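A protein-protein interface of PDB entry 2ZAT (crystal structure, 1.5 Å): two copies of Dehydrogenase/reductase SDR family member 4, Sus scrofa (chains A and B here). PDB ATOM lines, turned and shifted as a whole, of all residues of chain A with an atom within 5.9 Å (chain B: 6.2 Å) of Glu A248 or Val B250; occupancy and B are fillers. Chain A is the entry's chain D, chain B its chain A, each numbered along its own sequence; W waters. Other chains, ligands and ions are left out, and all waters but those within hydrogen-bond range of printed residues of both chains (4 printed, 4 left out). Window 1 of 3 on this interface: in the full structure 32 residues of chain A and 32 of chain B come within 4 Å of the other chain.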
ATOM      1  N   THR A 175      28.567   6.026 -25.773  1.00  0.00           N
ATOM      2  CA  THR A 175      28.917   6.598 -24.480  1.00  0.00           C
ATOM      3  C   THR A 175      27.830   6.366 -23.454  1.00  0.00           C
ATOM      4  O   THR A 175      28.091   5.935 -22.328  1.00  0.00           O
ATOM      5  CB  THR A 175      29.208   8.096 -24.633  1.00  0.00           C
ATOM      6  OG1 THR A 175      30.324   8.277 -25.508  1.00  0.00           O
ATOM      7  CG2 THR A 175      29.643   8.731 -23.301  1.00  0.00           C
ATOM      8  N   LYS A 176      26.608   6.711 -23.805  1.00  0.00           N
ATOM      9  CA  LYS A 176      25.493   6.552 -22.909  1.00  0.00           C
ATOM     10  C   LYS A 176      25.278   5.103 -22.497  1.00  0.00           C
ATOM     11  O   LYS A 176      25.005   4.817 -21.328  1.00  0.00           O
ATOM     12  CB  LYS A 176      24.203   7.071 -23.548  1.00  0.00           C
ATOM     13  CG  LYS A 176      24.154   8.552 -23.795  1.00  0.00           C
ATOM     14  CD  LYS A 176      24.042   9.322 -22.522  1.00  0.00           C
ATOM     15  CE  LYS A 176      23.655  10.763 -22.768  1.00  0.00           C
ATOM     16  NZ  LYS A 176      23.597  11.496 -21.460  1.00  0.00           N
ATOM     17  N   ALA A 179      28.134   3.926 -20.230  1.00  0.00           N
ATOM     18  CA  ALA A 179      28.087   4.524 -18.899  1.00  0.00           C
ATOM     19  C   ALA A 179      27.071   3.810 -18.025  1.00  0.00           C
ATOM     20  O   ALA A 179      27.362   3.554 -16.876  1.00  0.00           O
ATOM     21  CB  ALA A 179      27.739   5.989 -18.993  1.00  0.00           C
ATOM     22  N   VAL A 189      32.138   6.628 -17.975  1.00  0.00           N
ATOM     23  CA  VAL A 189      32.339   6.750 -19.425  1.00  0.00           C
ATOM     24  C   VAL A 189      31.749   8.056 -19.887  1.00  0.00           C
ATOM     25  O   VAL A 189      30.572   8.324 -19.690  1.00  0.00           O
ATOM     26  CB  VAL A 189      31.697   5.609 -20.220  1.00  0.00           C
ATOM     27  CG1 VAL A 189      32.061   5.692 -21.653  1.00  0.00           C
ATOM     28  CG2 VAL A 189      32.097   4.256 -19.622  1.00  0.00           C
ATOM     29  N   ASN A 190      32.583   8.897 -20.491  1.00  0.00           N
ATOM     30  CA  ASN A 190      32.208  10.216 -20.956  1.00  0.00           C
ATOM     31  C   ASN A 190      32.761  10.416 -22.335  1.00  0.00           C
ATOM     32  O   ASN A 190      33.489   9.574 -22.863  1.00  0.00           O
ATOM     33  CB  ASN A 190      32.714  11.285 -19.992  1.00  0.00           C
ATOM     34  CG  ASN A 190      32.067  11.184 -18.607  1.00  0.00           C
ATOM     35  OD1 ASN A 190      30.883  11.442 -18.459  1.00  0.00           O
ATOM     36  ND2 ASN A 190      32.872  10.850 -17.579  1.00  0.00           N
ATOM     37  N   CYS A 191      32.413  11.546 -22.944  1.00  0.00           N
ATOM     38  CA  CYS A 191      32.739  11.802 -24.330  1.00  0.00           C
ATOM     39  C   CYS A 191      33.157  13.263 -24.498  1.00  0.00           C
ATOM     40  O   CYS A 191      32.568  14.164 -23.896  1.00  0.00           O
ATOM     41  CB  CYS A 191      31.490  11.514 -25.164  1.00  0.00           C
ATOM     42  SG  CYS A 191      31.616  11.900 -26.928  1.00  0.00           S
ATOM     43  N   LEU A 192      34.168  13.467 -25.331  1.00  0.00           N
ATOM     44  CA  LEU A 192      34.624  14.781 -25.766  1.00  0.00           C
ATOM     45  C   LEU A 192      34.171  14.968 -27.191  1.00  0.00           C
ATOM     46  O   LEU A 192      34.447  14.121 -28.028  1.00  0.00           O
ATOM     47  CB  LEU A 192      36.147  14.816 -25.737  1.00  0.00           C
ATOM     48  CG  LEU A 192      36.837  15.966 -26.485  1.00  0.00           C
ATOM     49  CD1 LEU A 192      36.537  17.329 -25.871  1.00  0.00           C
ATOM     50  CD2 LEU A 192      38.336  15.770 -26.610  1.00  0.00           C
ATOM     51  N   LEU A 237      37.949  15.012 -16.506  1.00  0.00           N
ATOM     52  CA  LEU A 237      36.963  13.934 -16.522  1.00  0.00           C
ATOM     53  C   LEU A 237      37.568  12.591 -16.138  1.00  0.00           C
ATOM     54  O   LEU A 237      36.844  11.705 -15.687  1.00  0.00           O
ATOM     55  CB  LEU A 237      36.273  13.840 -17.877  1.00  0.00           C
ATOM     56  CG  LEU A 237      35.338  14.990 -18.208  1.00  0.00           C
ATOM     57  CD1 LEU A 237      34.913  14.898 -19.683  1.00  0.00           C
ATOM     58  CD2 LEU A 237      34.162  14.997 -17.258  1.00  0.00           C
ATOM     59  N   ILE A 245      30.393  12.361 -12.459  1.00  0.00           N
ATOM     60  CA  ILE A 245      30.139  12.664 -13.868  1.00  0.00           C
ATOM     61  C   ILE A 245      30.359  11.423 -14.722  1.00  0.00           C
ATOM     62  O   ILE A 245      31.492  10.916 -14.834  1.00  0.00           O
ATOM     63  CB  ILE A 245      31.055  13.795 -14.377  1.00  0.00           C
ATOM     64  CG1 ILE A 245      30.919  15.023 -13.494  1.00  0.00           C
ATOM     65  CG2 ILE A 245      30.696  14.174 -15.838  1.00  0.00           C
ATOM     66  CD1 ILE A 245      31.816  16.178 -13.887  1.00  0.00           C
ATOM     67  N   THR A 246      29.283  10.891 -15.268  1.00  0.00           N
ATOM     68  CA  THR A 246      29.332   9.770 -16.198  1.00  0.00           C
ATOM     69  C   THR A 246      28.214   9.915 -17.213  1.00  0.00           C
ATOM     70  O   THR A 246      27.163  10.507 -16.927  1.00  0.00           O
ATOM     71  CB  THR A 246      29.312   8.432 -15.464  1.00  0.00           C
ATOM     72  OG1 THR A 246      29.685   7.395 -16.374  1.00  0.00           O
ATOM     73  CG2 THR A 246      27.941   8.110 -14.913  1.00  0.00           C
ATOM     74  N   GLY A 247      28.438   9.369 -18.401  1.00  0.00           N
ATOM     75  CA  GLY A 247      27.470   9.431 -19.474  1.00  0.00           C
ATOM     76  C   GLY A 247      27.330  10.804 -20.079  1.00  0.00           C
ATOM     77  O   GLY A 247      26.311  11.067 -20.737  1.00  0.00           O
ATOM     78  N   GLU A 248      28.314  11.658 -19.910  1.00  0.00           N
ATOM     79  CA  GLU A 248      28.247  13.060 -20.334  1.00  0.00           C
ATOM     80  C   GLU A 248      29.136  13.318 -21.535  1.00  0.00           C
ATOM     81  O   GLU A 248      30.250  12.818 -21.592  1.00  0.00           O
ATOM     82  CB  GLU A 248      28.732  13.923 -19.177  1.00  0.00           C
ATOM     83  CG  GLU A 248      28.535  15.414 -19.248  1.00  0.00           C
ATOM     84  CD  GLU A 248      27.072  15.819 -19.306  1.00  0.00           C
ATOM     85  OE1 GLU A 248      26.179  14.917 -19.119  1.00  0.00           O
ATOM     86  OE2 GLU A 248      26.815  17.034 -19.608  1.00  0.00           O
ATOM     87  N   THR A 249      28.645  14.111 -22.477  1.00  0.00           N
ATOM     88  CA  THR A 249      29.428  14.603 -23.591  1.00  0.00           C
ATOM     89  C   THR A 249      29.685  16.077 -23.322  1.00  0.00           C
ATOM     90  O   THR A 249      28.752  16.824 -23.042  1.00  0.00           O
ATOM     91  CB  THR A 249      28.697  14.396 -24.939  1.00  0.00           C
ATOM     92  OG1 THR A 249      28.562  12.993 -25.175  1.00  0.00           O
ATOM     93  CG2 THR A 249      29.516  14.951 -26.104  1.00  0.00           C
ATOM     94  N   VAL A 250      30.923  16.494 -23.430  1.00  0.00           N
ATOM     95  CA  VAL A 250      31.322  17.887 -23.343  1.00  0.00           C
ATOM     96  C   VAL A 250      31.832  18.360 -24.692  1.00  0.00           C
ATOM     97  O   VAL A 250      32.778  17.812 -25.250  1.00  0.00           O
ATOM     98  CB  VAL A 250      32.382  18.133 -22.250  1.00  0.00           C
ATOM     99  CG1 VAL A 250      32.650  19.601 -22.134  1.00  0.00           C
ATOM    100  CG2 VAL A 250      31.934  17.634 -20.915  1.00  0.00           C
ATOM    101  N   ARG A 259      23.936  21.576 -28.803  1.00  0.00           N
ATOM    102  CA  ARG A 259      22.622  21.191 -28.300  1.00  0.00           C
ATOM    103  C   ARG A 259      22.339  21.805 -26.934  1.00  0.00           C
ATOM    104  O   ARG A 259      23.264  22.192 -26.233  1.00  0.00           O
ATOM    105  CB  ARG A 259      22.465  19.679 -28.262  1.00  0.00           C
ATOM    106  CG  ARG A 259      22.971  18.955 -27.094  1.00  0.00           C
ATOM    107  CD  ARG A 259      24.408  19.008 -26.899  1.00  0.00           C
ATOM    108  NE  ARG A 259      24.746  17.979 -25.944  1.00  0.00           N
ATOM    109  CZ  ARG A 259      25.804  17.981 -25.145  1.00  0.00           C
ATOM    110  NH1 ARG A 259      26.701  18.938 -25.169  1.00  0.00           N
ATOM    111  NH2 ARG A 259      25.968  16.940 -24.363  1.00  0.00           N
ATOM    112  N   TYR B 155      16.020  19.060 -18.108  1.00  0.00           N
ATOM    113  CA  TYR B 155      15.917  18.074 -19.203  1.00  0.00           C
ATOM    114  C   TYR B 155      14.874  17.020 -18.915  1.00  0.00           C
ATOM    115  O   TYR B 155      14.183  16.570 -19.849  1.00  0.00           O
ATOM    116  CB  TYR B 155      17.252  17.386 -19.349  1.00  0.00           C
ATOM    117  CG  TYR B 155      18.380  18.288 -19.736  1.00  0.00           C
ATOM    118  CD1 TYR B 155      19.374  18.637 -18.818  1.00  0.00           C
ATOM    119  CD2 TYR B 155      18.530  18.741 -21.045  1.00  0.00           C
ATOM    120  CE1 TYR B 155      20.420  19.455 -19.170  1.00  0.00           C
ATOM    121  CE2 TYR B 155      19.573  19.541 -21.405  1.00  0.00           C
ATOM    122  CZ  TYR B 155      20.553  19.876 -20.465  1.00  0.00           C
ATOM    123  OH  TYR B 155      21.589  20.673 -20.826  1.00  0.00           O
ATOM    124  N   CYS B 191      27.055  26.426 -18.043  1.00  0.00           N
ATOM    125  CA  CYS B 191      26.002  26.063 -17.093  1.00  0.00           C
ATOM    126  C   CYS B 191      26.319  24.733 -16.446  1.00  0.00           C
ATOM    127  O   CYS B 191      26.813  23.825 -17.104  1.00  0.00           O
ATOM    128  CB  CYS B 191      24.687  26.051 -17.825  1.00  0.00           C
ATOM    129  SG  CYS B 191      23.237  25.427 -16.948  1.00  0.00           S
ATOM    130  N   LEU B 192      26.068  24.631 -15.141  1.00  0.00           N
ATOM    131  CA  LEU B 192      26.164  23.402 -14.367  1.00  0.00           C
ATOM    132  C   LEU B 192      24.736  22.926 -14.135  1.00  0.00           C
ATOM    133  O   LEU B 192      23.917  23.678 -13.606  1.00  0.00           O
ATOM    134  CB  LEU B 192      26.828  23.680 -13.015  1.00  0.00           C
ATOM    135  CG  LEU B 192      26.653  22.634 -11.899  1.00  0.00           C
ATOM    136  CD1 LEU B 192      27.387  21.371 -12.277  1.00  0.00           C
ATOM    137  CD2 LEU B 192      27.086  23.163 -10.541  1.00  0.00           C
ATOM    138  N   ALA B 193      24.433  21.666 -14.451  1.00  0.00           N
ATOM    139  CA  ALA B 193      23.124  21.075 -14.196  1.00  0.00           C
ATOM    140  C   ALA B 193      23.284  19.899 -13.234  1.00  0.00           C
ATOM    141  O   ALA B 193      23.506  18.755 -13.664  1.00  0.00           O
ATOM    142  CB  ALA B 193      22.506  20.648 -15.499  1.00  0.00           C
ATOM    143  N   PRO B 194      23.188  20.149 -11.933  1.00  0.00           N
ATOM    144  CA  PRO B 194      23.336  19.053 -10.973  1.00  0.00           C
ATOM    145  C   PRO B 194      22.153  18.093 -11.017  1.00  0.00           C
ATOM    146  O   PRO B 194      21.050  18.493 -11.305  1.00  0.00           O
ATOM    147  CB  PRO B 194      23.399  19.782  -9.628  1.00  0.00           C
ATOM    148  CG  PRO B 194      23.709  21.160  -9.960  1.00  0.00           C
ATOM    149  CD  PRO B 194      22.983  21.441 -11.247  1.00  0.00           C
ATOM    150  N   ILE B 233      34.210  20.873 -11.611  1.00  0.00           N
ATOM    151  CA  ILE B 233      33.887  21.269 -12.972  1.00  0.00           C
ATOM    152  C   ILE B 233      33.682  22.785 -13.048  1.00  0.00           C
ATOM    153  O   ILE B 233      34.012  23.403 -14.044  1.00  0.00           O
ATOM    154  CB  ILE B 233      32.676  20.460 -13.533  1.00  0.00           C
ATOM    155  CG1 ILE B 233      32.401  20.773 -15.007  1.00  0.00           C
ATOM    156  CG2 ILE B 233      31.414  20.709 -12.735  1.00  0.00           C
ATOM    157  CD1 ILE B 233      33.512  20.351 -15.911  1.00  0.00           C
ATOM    158  N   LEU B 237      35.830  25.220 -15.461  1.00  0.00           N
ATOM    159  CA  LEU B 237      35.163  26.049 -16.473  1.00  0.00           C
ATOM    160  C   LEU B 237      35.441  27.516 -16.298  1.00  0.00           C
ATOM    161  O   LEU B 237      35.375  28.277 -17.264  1.00  0.00           O
ATOM    162  CB  LEU B 237      33.659  25.799 -16.487  1.00  0.00           C
ATOM    163  CG  LEU B 237      33.251  24.418 -17.058  1.00  0.00           C
ATOM    164  CD1 LEU B 237      31.760  24.206 -16.807  1.00  0.00           C
ATOM    165  CD2 LEU B 237      33.616  24.276 -18.546  1.00  0.00           C
ATOM    166  N   GLU B 248      28.102  25.860 -22.997  1.00  0.00           N
ATOM    167  CA  GLU B 248      27.957  24.436 -22.663  1.00  0.00           C
ATOM    168  C   GLU B 248      27.281  24.245 -21.325  1.00  0.00           C
ATOM    169  O   GLU B 248      27.575  24.957 -20.354  1.00  0.00           O
ATOM    170  CB  GLU B 248      29.323  23.790 -22.612  1.00  0.00           C
ATOM    171  CG  GLU B 248      29.409  22.291 -22.531  1.00  0.00           C
ATOM    172  CD  GLU B 248      28.931  21.599 -23.798  1.00  0.00           C
ATOM    173  OE1 GLU B 248      28.535  22.302 -24.818  1.00  0.00           O
ATOM    174  OE2 GLU B 248      28.895  20.332 -23.729  1.00  0.00           O
ATOM    175  N   THR B 249      26.441  23.224 -21.248  1.00  0.00           N
ATOM    176  CA  THR B 249      25.875  22.759 -19.985  1.00  0.00           C
ATOM    177  C   THR B 249      26.517  21.438 -19.643  1.00  0.00           C
ATOM    178  O   THR B 249      26.579  20.549 -20.523  1.00  0.00           O
ATOM    179  CB  THR B 249      24.341  22.625 -20.074  1.00  0.00           C
ATOM    180  OG1 THR B 249      23.768  23.940 -20.244  1.00  0.00           O
ATOM    181  CG2 THR B 249      23.783  22.092 -18.744  1.00  0.00           C
ATOM    182  N   VAL B 250      27.011  21.280 -18.434  1.00  0.00           N
ATOM    183  CA  VAL B 250      27.561  20.034 -17.962  1.00  0.00           C
ATOM    184  C   VAL B 250      26.679  19.503 -16.866  1.00  0.00           C
ATOM    185  O   VAL B 250      26.470  20.158 -15.835  1.00  0.00           O
ATOM    186  CB  VAL B 250      29.021  20.170 -17.452  1.00  0.00           C
ATOM    187  CG1 VAL B 250      29.546  18.815 -17.056  1.00  0.00           C
ATOM    188  CG2 VAL B 250      29.928  20.817 -18.454  1.00  0.00           C
ATOM    189  N   VAL B 251      26.192  18.282 -17.049  1.00  0.00           N
ATOM    190  CA  VAL B 251      25.386  17.589 -16.067  1.00  0.00           C
ATOM    191  C   VAL B 251      26.293  16.833 -15.116  1.00  0.00           C
ATOM    192  O   VAL B 251      27.235  16.159 -15.564  1.00  0.00           O
ATOM    193  CB  VAL B 251      24.455  16.606 -16.771  1.00  0.00           C
ATOM    194  CG1 VAL B 251      23.736  15.729 -15.808  1.00  0.00           C
ATOM    195  CG2 VAL B 251      23.433  17.372 -17.602  1.00  0.00           C
ATOM    196  N   VAL B 252      26.055  17.018 -13.826  1.00  0.00           N
ATOM    197  CA  VAL B 252      26.777  16.337 -12.767  1.00  0.00           C
ATOM    198  C   VAL B 252      25.723  15.546 -12.011  1.00  0.00           C
ATOM    199  O   VAL B 252      25.133  16.000 -11.031  1.00  0.00           O
ATOM    200  CB  VAL B 252      27.507  17.336 -11.850  1.00  0.00           C
ATOM    201  CG1 VAL B 252      28.249  16.608 -10.754  1.00  0.00           C
ATOM    202  CG2 VAL B 252      28.512  18.115 -12.684  1.00  0.00           C
ATOM    203  N   SER B 258      19.800  12.547 -18.893  1.00  0.00           N
ATOM    204  CA  SER B 258      19.721  13.966 -19.230  1.00  0.00           C
ATOM    205  C   SER B 258      19.415  14.100 -20.715  1.00  0.00           C
ATOM    206  O   SER B 258      18.250  14.201 -21.096  1.00  0.00           O
ATOM    207  CB  SER B 258      21.009  14.713 -18.827  1.00  0.00           C
ATOM    208  OG  SER B 258      22.189  14.157 -19.405  1.00  0.00           O
ATOM    209  N   ARG B 259      20.460  14.079 -21.545  1.00  0.00           N
ATOM    210  CA  ARG B 259      20.305  14.244 -22.985  1.00  0.00           C
ATOM    211  C   ARG B 259      21.543  13.762 -23.723  1.00  0.00           C
ATOM    212  O   ARG B 259      22.625  13.653 -23.139  1.00  0.00           O
ATOM    213  CB  ARG B 259      20.001  15.693 -23.352  1.00  0.00           C
ATOM    214  CG  ARG B 259      21.168  16.578 -23.558  1.00  0.00           C
ATOM    215  CD  ARG B 259      21.890  16.923 -22.328  1.00  0.00           C
ATOM    216  NE  ARG B 259      22.658  18.124 -22.597  1.00  0.00           N
ATOM    217  CZ  ARG B 259      23.783  18.473 -21.994  1.00  0.00           C
ATOM    218  NH1 ARG B 259      24.374  17.717 -21.089  1.00  0.00           N
ATOM    219  NH2 ARG B 259      24.329  19.617 -22.356  1.00  0.00           N
HETATM  220  O   HOH W   1      23.183  11.780 -18.412  1.00  0.00           O
HETATM  221  O   HOH W   2      25.100  22.157 -23.727  1.00  0.00           O
HETATM  222  O   HOH W   3      26.982  13.394 -14.985  1.00  0.00           O
HETATM  223  O   HOH W   4      25.623  14.392 -22.673  1.00  0.00           O
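The backbone NH of Cys B191 is in hydrogen-bond range of the backbone carbonyl oxygen of Glu B248 (2.8 Å).
N of Ala B193 is in hydrogen-bond range of O of Val B250 (2.9 Å).
O of Thr B249 lies within hydrogen-bond range of NH2 of Arg B259.
O of Gly A247 lies within hydrogen-bond range of NZ of Lys A176, 2.8 Å away.
The side-chain amide nitrogen (ND2) of Asn A190 lies within hydrogen-bond range of the backbone carbonyl oxygen (O) of Ile A245, at 3.1 Å.
The side-chain amide oxygen (OD1) of Asn A190 sits at hydrogen-bond distance from the backbone NH (N) of Glu A248.
Among the printed residues, pairs that only touch across the chains: Val A250 with Glu B248 (3.5 Å), Glu A248 with Val B250 (3.5 Å), Arg A259 with Arg B259 (3.6 Å), Thr A249 with Glu B248 (3.6 Å), Glu A248 with Thr B249 (3.6 Å), Lys A176 with Ser B258 (3.6 Å) and Ile A245 with Val B251 (3.999 Å).
The side-chain carboxylate (OE2) of Glu B248 lies within salt-bridge range of the guanidinium group (NH1) of Arg A259, 3.0 Å away.
The side-chain carboxylate of Glu A248 sits at hydrogen-bond distance from the backbone NH of Val B251 (2.9 Å).
NZ of Lys A176 sits at hydrogen-bond distance from O of Arg B259 (2.9 Å).
The side-chain carboxylate of Glu A248 lies within salt-bridge range of the guanidinium group of Arg B259, 2.9 Å away.
Glu A248 touches just these residues of chain B: Thr B249, Val B250, Val B251 and Arg B259.
Val B250 touches one residue of chain A.
Of the printed residues of chain B, Arg A259 touches Glu B248 (3.0 Å) and Arg B259 (3.6 Å).
Of the printed residues of chain B, Val A250 touches Glu B248 (3.5 Å).
Of the printed residues of chain A, Glu B248 touches Thr A249 (3.6 Å), Val A250 (3.5 Å) and Arg A259 (3.0 Å).
Of the printed residues of chain B, Ile A245 touches Val B251 (3.999 Å).
Of the printed residues of chain B, Thr A249 touches Glu B248.
Water W1 lies within hydrogen-bond range of the side-chain hydroxyl (OG) of Ser B258 (2.8 Å) and the side-chain amino group (NZ) of Lys A176 (3.1 Å).
Water W3 bridges O of Val B251 (2.8 Å) and N of Thr A246 (3.4 Å).
Water W2 lies within hydrogen-bond range of NH2 of Arg B259, N of Thr B249 and O of Arg A259.
Water W4 lies within hydrogen-bond range of N of Thr A249 (3.0 Å), NH2 of Arg A259 (3.1 Å) and O of Arg B259 (3.1 Å).
Glu A248 touches Thr B249, and with the chains exchanged Thr A249 touches Glu B248.
Glu A248 touches Val B250, and with the chains exchanged Val A250 touches Glu B248.
Glu A248 touches Arg B259, and with the chains exchanged Arg A259 touches Glu B248.
Arg A259 touches its own counterpart, Arg B259.
Of the 11 pairs that touch across the chains among the printed residues, 7 have their exchanged pair printed and touching as well.
Of the 15 printed residues of chain A, 6 touch a printed residue of chain B.
Hydrophobic or aromatic side chains of chain A that line the printed part of chain B: Ile A245.
Among the printed residues, Asp or Glu carboxylates within 4 Å of a Lys or Arg side-chain nitrogen of the other chain: Glu A248 with Arg B259 and Arg A259 with Glu B248.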
